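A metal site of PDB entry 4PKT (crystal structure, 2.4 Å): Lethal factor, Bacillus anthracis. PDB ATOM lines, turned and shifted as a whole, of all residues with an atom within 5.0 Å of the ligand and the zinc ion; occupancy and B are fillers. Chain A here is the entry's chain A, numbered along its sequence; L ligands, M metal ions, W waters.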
ATOM      1  N   ASP A  64      17.924  18.178 -32.163  1.00  0.00           N
ATOM      2  CA  ASP A  64      16.932  18.452 -31.125  1.00  0.00           C
ATOM      3  C   ASP A  64      17.562  18.902 -29.809  1.00  0.00           C
ATOM      4  O   ASP A  64      16.870  19.422 -28.921  1.00  0.00           O
ATOM      5  CB  ASP A  64      16.056  17.210 -30.889  1.00  0.00           C
ATOM      6  CG  ASP A  64      14.966  17.057 -31.934  1.00  0.00           C
ATOM      7  OD1 ASP A  64      14.708  18.034 -32.665  1.00  0.00           O
ATOM      8  OD2 ASP A  64      14.380  15.957 -32.014  1.00  0.00           O
ATOM      9  N   SER A  66      19.427  21.365 -29.339  1.00  0.00           N
ATOM     10  CA  SER A  66      19.778  22.775 -29.451  1.00  0.00           C
ATOM     11  C   SER A  66      18.825  23.614 -28.622  1.00  0.00           C
ATOM     12  O   SER A  66      17.619  23.388 -28.638  1.00  0.00           O
ATOM     13  CB  SER A  66      19.758  23.213 -30.915  1.00  0.00           C
ATOM     14  OG  SER A  66      20.116  24.584 -31.044  1.00  0.00           O
ATOM     15  N   ASP A  67      19.362  24.589 -27.885  1.00  0.00           N
ATOM     16  CA  ASP A  67      18.533  25.423 -27.007  1.00  0.00           C
ATOM     17  C   ASP A  67      18.283  26.820 -27.569  1.00  0.00           C
ATOM     18  O   ASP A  67      17.755  27.694 -26.869  1.00  0.00           O
ATOM     19  CB  ASP A  67      19.161  25.520 -25.607  1.00  0.00           C
ATOM     20  CG  ASP A  67      20.561  26.130 -25.613  1.00  0.00           C
ATOM     21  OD1 ASP A  67      21.175  26.252 -26.700  1.00  0.00           O
ATOM     22  OD2 ASP A  67      21.049  26.477 -24.522  1.00  0.00           O
ATOM     23  N   LYS A  74      14.319  23.494 -36.275  1.00  0.00           N
ATOM     24  CA  LYS A  74      14.866  22.162 -36.026  1.00  0.00           C
ATOM     25  C   LYS A  74      14.408  21.171 -37.103  1.00  0.00           C
ATOM     26  O   LYS A  74      15.173  20.312 -37.516  1.00  0.00           O
ATOM     27  CB  LYS A  74      14.461  21.669 -34.627  1.00  0.00           C
ATOM     28  CG  LYS A  74      15.207  22.357 -33.483  1.00  0.00           C
ATOM     29  CD  LYS A  74      14.707  21.920 -32.112  1.00  0.00           C
ATOM     30  CE  LYS A  74      15.586  22.499 -31.004  1.00  0.00           C
ATOM     31  NZ  LYS A  74      15.123  22.148 -29.636  1.00  0.00           N
ATOM     32  N   SER A 394      13.451  32.338 -27.020  1.00  0.00           N
ATOM     33  CA  SER A 394      13.117  31.241 -26.137  1.00  0.00           C
ATOM     34  C   SER A 394      12.004  31.687 -25.210  1.00  0.00           C
ATOM     35  O   SER A 394      11.498  32.802 -25.328  1.00  0.00           O
ATOM     36  CB  SER A 394      14.331  30.794 -25.313  1.00  0.00           C
ATOM     37  OG  SER A 394      14.816  31.856 -24.507  1.00  0.00           O
ATOM     38  N   LYS A 395      11.630  30.795 -24.296  1.00  0.00           N
ATOM     39  CA  LYS A 395      10.562  31.062 -23.348  1.00  0.00           C
ATOM     40  C   LYS A 395      10.968  32.168 -22.402  1.00  0.00           C
ATOM     41  O   LYS A 395      10.167  33.034 -22.042  1.00  0.00           O
ATOM     42  CB  LYS A 395      10.222  29.800 -22.556  1.00  0.00           C
ATOM     43  CG  LYS A 395       9.080  29.992 -21.589  1.00  0.00           C
ATOM     44  CD  LYS A 395       7.800  30.249 -22.395  1.00  0.00           C
ATOM     45  CE  LYS A 395       6.658  30.610 -21.500  1.00  0.00           C
ATOM     46  NZ  LYS A 395       5.412  30.825 -22.265  1.00  0.00           N
ATOM     47  N   GLY A 396      12.229  32.151 -21.981  1.00  0.00           N
ATOM     48  CA  GLY A 396      12.691  33.089 -20.980  1.00  0.00           C
ATOM     49  C   GLY A 396      14.194  33.300 -21.062  1.00  0.00           C
ATOM     50  O   GLY A 396      14.935  32.477 -21.609  1.00  0.00           O
ATOM     51  N   LEU A 397      14.645  34.407 -20.494  1.00  0.00           N
ATOM     52  CA  LEU A 397      16.044  34.775 -20.587  1.00  0.00           C
ATOM     53  C   LEU A 397      16.414  35.715 -19.424  1.00  0.00           C
ATOM     54  O   LEU A 397      15.593  36.504 -18.941  1.00  0.00           O
ATOM     55  CB  LEU A 397      16.310  35.455 -21.953  1.00  0.00           C
ATOM     56  CG  LEU A 397      17.655  35.258 -22.674  1.00  0.00           C
ATOM     57  CD1 LEU A 397      17.903  33.780 -22.949  1.00  0.00           C
ATOM     58  CD2 LEU A 397      17.667  36.055 -23.997  1.00  0.00           C
ATOM     59  N   TYR A 398      17.668  35.627 -18.982  1.00  0.00           N
ATOM     60  CA  TYR A 398      18.215  36.663 -18.127  1.00  0.00           C
ATOM     61  C   TYR A 398      19.387  37.291 -18.852  1.00  0.00           C
ATOM     62  O   TYR A 398      20.277  36.588 -19.326  1.00  0.00           O
ATOM     63  CB  TYR A 398      18.643  36.109 -16.754  1.00  0.00           C
ATOM     64  CG  TYR A 398      19.332  37.161 -15.915  1.00  0.00           C
ATOM     65  CD1 TYR A 398      18.615  38.224 -15.377  1.00  0.00           C
ATOM     66  CD2 TYR A 398      20.700  37.123 -15.678  1.00  0.00           C
ATOM     67  CE1 TYR A 398      19.216  39.205 -14.647  1.00  0.00           C
ATOM     68  CE2 TYR A 398      21.318  38.115 -14.928  1.00  0.00           C
ATOM     69  CZ  TYR A 398      20.571  39.155 -14.422  1.00  0.00           C
ATOM     70  OH  TYR A 398      21.146  40.163 -13.675  1.00  0.00           O
ATOM     71  N   GLY A 413       7.920  26.456 -22.974  1.00  0.00           N
ATOM     72  CA  GLY A 413       9.296  26.120 -22.648  1.00  0.00           C
ATOM     73  C   GLY A 413       9.509  24.630 -22.684  1.00  0.00           C
ATOM     74  O   GLY A 413       8.637  23.862 -22.301  1.00  0.00           O
ATOM     75  N   VAL A 414      10.679  24.209 -23.143  1.00  0.00           N
ATOM     76  CA  VAL A 414      11.006  22.790 -23.189  1.00  0.00           C
ATOM     77  C   VAL A 414      11.115  22.201 -21.774  1.00  0.00           C
ATOM     78  O   VAL A 414      11.982  22.592 -20.984  1.00  0.00           O
ATOM     79  CB  VAL A 414      12.299  22.515 -23.966  1.00  0.00           C
ATOM     80  CG1 VAL A 414      12.738  21.069 -23.769  1.00  0.00           C
ATOM     81  CG2 VAL A 414      12.107  22.828 -25.444  1.00  0.00           C
ATOM     82  N   GLU A 415      10.223  21.256 -21.493  1.00  0.00           N
ATOM     83  CA  GLU A 415      10.091  20.616 -20.187  1.00  0.00           C
ATOM     84  C   GLU A 415       9.806  21.618 -19.075  1.00  0.00           C
ATOM     85  O   GLU A 415      10.350  21.501 -17.980  1.00  0.00           O
ATOM     86  CB  GLU A 415      11.339  19.806 -19.858  1.00  0.00           C
ATOM     87  CG  GLU A 415      11.517  18.590 -20.759  1.00  0.00           C
ATOM     88  CD  GLU A 415      10.587  17.437 -20.386  1.00  0.00           C
ATOM     89  OE1 GLU A 415      10.932  16.653 -19.468  1.00  0.00           O
ATOM     90  OE2 GLU A 415       9.503  17.326 -21.008  1.00  0.00           O
ATOM     91  N   LEU A 416       8.937  22.589 -19.353  1.00  0.00           N
ATOM     92  CA  LEU A 416       8.458  23.531 -18.346  1.00  0.00           C
ATOM     93  C   LEU A 416       6.938  23.428 -18.176  1.00  0.00           C
ATOM     94  O   LEU A 416       6.212  23.541 -19.150  1.00  0.00           O
ATOM     95  CB  LEU A 416       8.831  24.963 -18.712  1.00  0.00           C
ATOM     96  CG  LEU A 416       9.999  25.682 -18.064  1.00  0.00           C
ATOM     97  CD1 LEU A 416      10.061  27.142 -18.589  1.00  0.00           C
ATOM     98  CD2 LEU A 416       9.902  25.645 -16.553  1.00  0.00           C
ATOM     99  N   GLU A 421       7.146  28.799 -13.325  1.00  0.00           N
ATOM    100  CA  GLU A 421       8.380  28.050 -13.092  1.00  0.00           C
ATOM    101  C   GLU A 421       9.528  28.636 -13.913  1.00  0.00           C
ATOM    102  O   GLU A 421      10.658  28.701 -13.444  1.00  0.00           O
ATOM    103  CB  GLU A 421       8.183  26.552 -13.413  1.00  0.00           C
ATOM    104  CG  GLU A 421       7.362  25.832 -12.353  1.00  0.00           C
ATOM    105  CD  GLU A 421       7.357  24.316 -12.531  1.00  0.00           C
ATOM    106  OE1 GLU A 421       7.627  23.838 -13.661  1.00  0.00           O
ATOM    107  OE2 GLU A 421       7.088  23.607 -11.528  1.00  0.00           O
ATOM    108  N   GLY A 422       9.216  29.076 -15.130  1.00  0.00           N
ATOM    109  CA  GLY A 422      10.209  29.664 -16.003  1.00  0.00           C
ATOM    110  C   GLY A 422      10.817  30.930 -15.416  1.00  0.00           C
ATOM    111  O   GLY A 422      12.026  31.141 -15.473  1.00  0.00           O
ATOM    112  N   HIS A 425      13.304  30.162 -12.657  1.00  0.00           N
ATOM    113  CA  HIS A 425      14.586  29.771 -13.251  1.00  0.00           C
ATOM    114  C   HIS A 425      15.384  31.016 -13.639  1.00  0.00           C
ATOM    115  O   HIS A 425      16.590  31.069 -13.353  1.00  0.00           O
ATOM    116  CB  HIS A 425      14.362  28.835 -14.458  1.00  0.00           C
ATOM    117  CG  HIS A 425      15.544  28.720 -15.387  1.00  0.00           C
ATOM    118  ND1 HIS A 425      16.271  27.569 -15.539  1.00  0.00           N
ATOM    119  CD2 HIS A 425      16.099  29.617 -16.256  1.00  0.00           C
ATOM    120  CE1 HIS A 425      17.233  27.753 -16.425  1.00  0.00           C
ATOM    121  NE2 HIS A 425      17.153  28.994 -16.873  1.00  0.00           N
ATOM    122  N   GLU A 426      14.740  31.998 -14.282  1.00  0.00           N
ATOM    123  CA  GLU A 426      15.498  33.180 -14.724  1.00  0.00           C
ATOM    124  C   GLU A 426      15.941  33.992 -13.519  1.00  0.00           C
ATOM    125  O   GLU A 426      17.037  34.539 -13.519  1.00  0.00           O
ATOM    126  CB  GLU A 426      14.671  34.075 -15.663  1.00  0.00           C
ATOM    127  CG  GLU A 426      13.954  33.366 -16.801  1.00  0.00           C
ATOM    128  CD  GLU A 426      14.886  32.646 -17.759  1.00  0.00           C
ATOM    129  OE1 GLU A 426      14.389  31.821 -18.542  1.00  0.00           O
ATOM    130  OE2 GLU A 426      16.112  32.908 -17.747  1.00  0.00           O
ATOM    131  N   HIS A 429      19.132  32.832 -12.403  1.00  0.00           N
ATOM    132  CA  HIS A 429      20.277  33.423 -13.089  1.00  0.00           C
ATOM    133  C   HIS A 429      20.671  34.768 -12.463  1.00  0.00           C
ATOM    134  O   HIS A 429      21.839  35.118 -12.368  1.00  0.00           O
ATOM    135  CB  HIS A 429      19.983  33.635 -14.571  1.00  0.00           C
ATOM    136  CG  HIS A 429      19.948  32.382 -15.397  1.00  0.00           C
ATOM    137  ND1 HIS A 429      21.030  31.516 -15.491  1.00  0.00           N
ATOM    138  CD2 HIS A 429      18.995  31.871 -16.214  1.00  0.00           C
ATOM    139  CE1 HIS A 429      20.724  30.532 -16.313  1.00  0.00           C
ATOM    140  NE2 HIS A 429      19.501  30.721 -16.762  1.00  0.00           N
ATOM    141  N   TYR A 467      18.616  19.273 -19.156  1.00  0.00           N
ATOM    142  CA  TYR A 467      19.092  20.593 -19.561  1.00  0.00           C
ATOM    143  C   TYR A 467      20.113  21.151 -18.548  1.00  0.00           C
ATOM    144  O   TYR A 467      20.976  21.946 -18.908  1.00  0.00           O
ATOM    145  CB  TYR A 467      17.909  21.546 -19.759  1.00  0.00           C
ATOM    146  CG  TYR A 467      18.328  22.931 -20.178  1.00  0.00           C
ATOM    147  CD1 TYR A 467      19.038  23.133 -21.344  1.00  0.00           C
ATOM    148  CD2 TYR A 467      18.035  24.035 -19.392  1.00  0.00           C
ATOM    149  CE1 TYR A 467      19.441  24.403 -21.734  1.00  0.00           C
ATOM    150  CE2 TYR A 467      18.420  25.302 -19.765  1.00  0.00           C
ATOM    151  CZ  TYR A 467      19.132  25.492 -20.937  1.00  0.00           C
ATOM    152  OH  TYR A 467      19.520  26.771 -21.318  1.00  0.00           O
ATOM    153  N   GLU A 474      23.297  27.204 -16.137  1.00  0.00           N
ATOM    154  CA  GLU A 474      21.991  26.586 -16.263  1.00  0.00           C
ATOM    155  C   GLU A 474      21.761  25.577 -15.137  1.00  0.00           C
ATOM    156  O   GLU A 474      20.659  25.500 -14.589  1.00  0.00           O
ATOM    157  CB  GLU A 474      21.812  25.898 -17.617  1.00  0.00           C
ATOM    158  CG  GLU A 474      22.013  26.785 -18.855  1.00  0.00           C
ATOM    159  CD  GLU A 474      21.118  28.019 -18.898  1.00  0.00           C
ATOM    160  OE1 GLU A 474      20.076  28.077 -18.222  1.00  0.00           O
ATOM    161  OE2 GLU A 474      21.474  28.968 -19.620  1.00  0.00           O
ATOM    162  N   ALA A 477      20.670  27.405 -12.216  1.00  0.00           N
ATOM    163  CA  ALA A 477      19.334  27.975 -12.415  1.00  0.00           C
ATOM    164  C   ALA A 477      18.281  26.886 -12.324  1.00  0.00           C
ATOM    165  O   ALA A 477      17.208  27.105 -11.768  1.00  0.00           O
ATOM    166  CB  ALA A 477      19.232  28.735 -13.793  1.00  0.00           C
ATOM    167  N   GLU A 478      18.580  25.719 -12.880  1.00  0.00           N
ATOM    168  CA  GLU A 478      17.662  24.591 -12.733  1.00  0.00           C
ATOM    169  C   GLU A 478      17.575  24.140 -11.264  1.00  0.00           C
ATOM    170  O   GLU A 478      16.479  23.941 -10.739  1.00  0.00           O
ATOM    171  CB  GLU A 478      18.079  23.432 -13.633  1.00  0.00           C
ATOM    172  CG  GLU A 478      17.756  23.664 -15.121  1.00  0.00           C
ATOM    173  CD  GLU A 478      16.253  23.596 -15.420  1.00  0.00           C
ATOM    174  OE1 GLU A 478      15.775  22.547 -15.936  1.00  0.00           O
ATOM    175  OE2 GLU A 478      15.536  24.587 -15.141  1.00  0.00           O
ATOM    176  N   ARG A 481      15.525  26.541  -9.388  1.00  0.00           N
ATOM    177  CA  ARG A 481      14.124  26.436  -9.743  1.00  0.00           C
ATOM    178  C   ARG A 481      13.504  25.219  -9.047  1.00  0.00           C
ATOM    179  O   ARG A 481      12.499  25.348  -8.356  1.00  0.00           O
ATOM    180  CB  ARG A 481      13.931  26.342 -11.267  1.00  0.00           C
ATOM    181  CG  ARG A 481      12.562  25.782 -11.651  1.00  0.00           C
ATOM    182  CD  ARG A 481      12.358  25.618 -13.141  1.00  0.00           C
ATOM    183  NE  ARG A 481      13.140  24.528 -13.720  1.00  0.00           N
ATOM    184  CZ  ARG A 481      12.687  23.277 -13.884  1.00  0.00           C
ATOM    185  NH1 ARG A 481      11.463  22.941 -13.492  1.00  0.00           N
ATOM    186  NH2 ARG A 481      13.468  22.370 -14.452  1.00  0.00           N
HETATM  187  C1  LIG L   1      15.898  23.280 -23.493  1.00  0.00           C
HETATM  188  C2  LIG L   1      16.064  24.339 -22.611  1.00  0.00           C
HETATM  189  C3  LIG L   1      15.704  23.527 -24.849  1.00  0.00           C
HETATM  190  C4  LIG L   1      15.668  24.848 -25.305  1.00  0.00           C
HETATM  191  C5  LIG L   1      15.842  25.927 -24.430  1.00  0.00           C
HETATM  192  C6  LIG L   1      16.036  25.656 -23.071  1.00  0.00           C
HETATM  193  C7  LIG L   1      16.232  26.745 -22.043  1.00  0.00           C
HETATM  194  N1  LIG L   1      15.400  27.941 -22.119  1.00  0.00           N
HETATM  195  C8  LIG L   1      16.256  29.158 -22.170  1.00  0.00           C
HETATM  196  C9  LIG L   1      17.346  29.002 -23.229  1.00  0.00           C
HETATM  197  C10 LIG L   1      16.954  29.563 -20.869  1.00  0.00           C
HETATM  198  N2  LIG L   1      16.911  30.846 -20.539  1.00  0.00           N
HETATM  199  O1  LIG L   1      17.409  31.249 -19.299  1.00  0.00           O
HETATM  200  O2  LIG L   1      17.567  28.771 -20.137  1.00  0.00           O
HETATM  201  S1  LIG L   1      13.843  27.894 -21.985  1.00  0.00           S
HETATM  202  O3  LIG L   1      13.183  26.892 -22.803  1.00  0.00           O
HETATM  203  O4  LIG L   1      13.287  29.197 -22.241  1.00  0.00           O
HETATM  204  C11 LIG L   1      13.689  27.538 -20.437  1.00  0.00           C
HETATM  205  C12 LIG L   1      13.726  28.579 -19.511  1.00  0.00           C
HETATM  206  C13 LIG L   1      13.627  28.276 -18.161  1.00  0.00           C
HETATM  207  C14 LIG L   1      13.512  26.954 -17.747  1.00  0.00           C
HETATM  208  F1  LIG L   1      13.401  26.701 -16.431  1.00  0.00           F
HETATM  209  C15 LIG L   1      13.488  25.901 -18.660  1.00  0.00           C
HETATM  210  C16 LIG L   1      13.586  26.194 -20.024  1.00  0.00           C
HETATM  211  C17 LIG L   1      13.372  24.476 -18.205  1.00  0.00           C
HETATM  212  N3  LIG L   1      15.535  22.432 -25.721  1.00  0.00           N
HETATM  213  O5  LIG L   1      15.329  22.629 -27.092  1.00  0.00           O
HETATM  214  O6  LIG L   1      15.570  21.128 -25.215  1.00  0.00           O
HETATM  215 ZN    ZN M   1      18.747  29.662 -18.325  1.00  0.00          ZN
HETATM  216  O   HOH W   1      19.378  33.169 -19.908  1.00  0.00           O
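The side-chain amino group of Lys 74 sits at hydrogen-bond distance from an oxygen (O5) of the ligand, at 2.6 Å. The side-chain carboxylate (OE1) of Glu 426 sits at hydrogen-bond distance from a nitrogen (N2) of the ligand. O4 of the ligand sits at hydrogen-bond distance from N of Gly 396, 3.1 Å away. O of Gly 396 sits at hydrogen-bond distance from N2 of the ligand (2.8 Å). An oxygen (O2) of the ligand lies close to the side-chain hydroxyl (OH) of Tyr 467 (3.0 Å). N of Lys 395 is in hydrogen-bond range of O4 of the ligand (3.1 Å).
The backbone carbonyl oxygen of Ser 66 lies close to an oxygen (O5) of the ligand, 2.9 Å away. A fluorine (F1) of the ligand lies close to the side-chain carboxylate (OE2) of Glu 478. A fluorine (F1) of the ligand lies close to the guanidinium group of Arg 481. Asp 67 touches the ligand (CA to C4, 3.4 Å). CB of Ser 394 touches O4 of the ligand, 3.6 Å away. CD1 of Leu 397 touches N2 of the ligand (3.9 Å). Gly 413 touches the ligand (CA to O3, 3.97 Å). CG1 of Val 414 touches O6 of the ligand, at 3.2 Å. Leu 416 touches the ligand (CG to C15, 3.5 Å). The nearest printed residue that does not touch the ligand is Asp 64 (4.001 Å).
A ring nitrogen (ND1) of His 425 lies within hydrogen-bond range of the side-chain carboxylate (OE2) of Glu 478. NZ of Lys 74 sits at hydrogen-bond distance from O of Ser 66 (3.0 Å). NZ of Lys 74 is in hydrogen-bond range of O of Asp 64, at 3.3 Å. N of Leu 397 is in hydrogen-bond range of OE1 of Glu 426 (3.3 Å). The side-chain carboxylate (OE2) of Glu 426 lies within hydrogen-bond range of the backbone NH (N) of Tyr 398, at 3.4 Å. OG of Ser 394 lies within hydrogen-bond range of O of Gly 396 (3.0 Å). NH2 of Arg 481 lies within salt-bridge range of OE1 of Glu 478, at 2.7 Å. The side-chain carboxylate (OE1) of Glu 421 lies within salt-bridge range of the guanidinium group (NH1) of Arg 481, at 3.9 Å.
The zinc ion is bound by a ring nitrogen (NE2) of His 429 (2.0 Å), the side-chain carboxylate of Glu 474 (2.1 Å), a ring nitrogen (NE2) of His 425 (2.3 Å), an oxygen (O1) of the ligand (2.3 Å) and an oxygen (O2) of the ligand (2.3 Å).
Water W1 lies within hydrogen-bond range of N of Tyr 398 (3.1 Å) and N2 of the ligand (3.4 Å).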
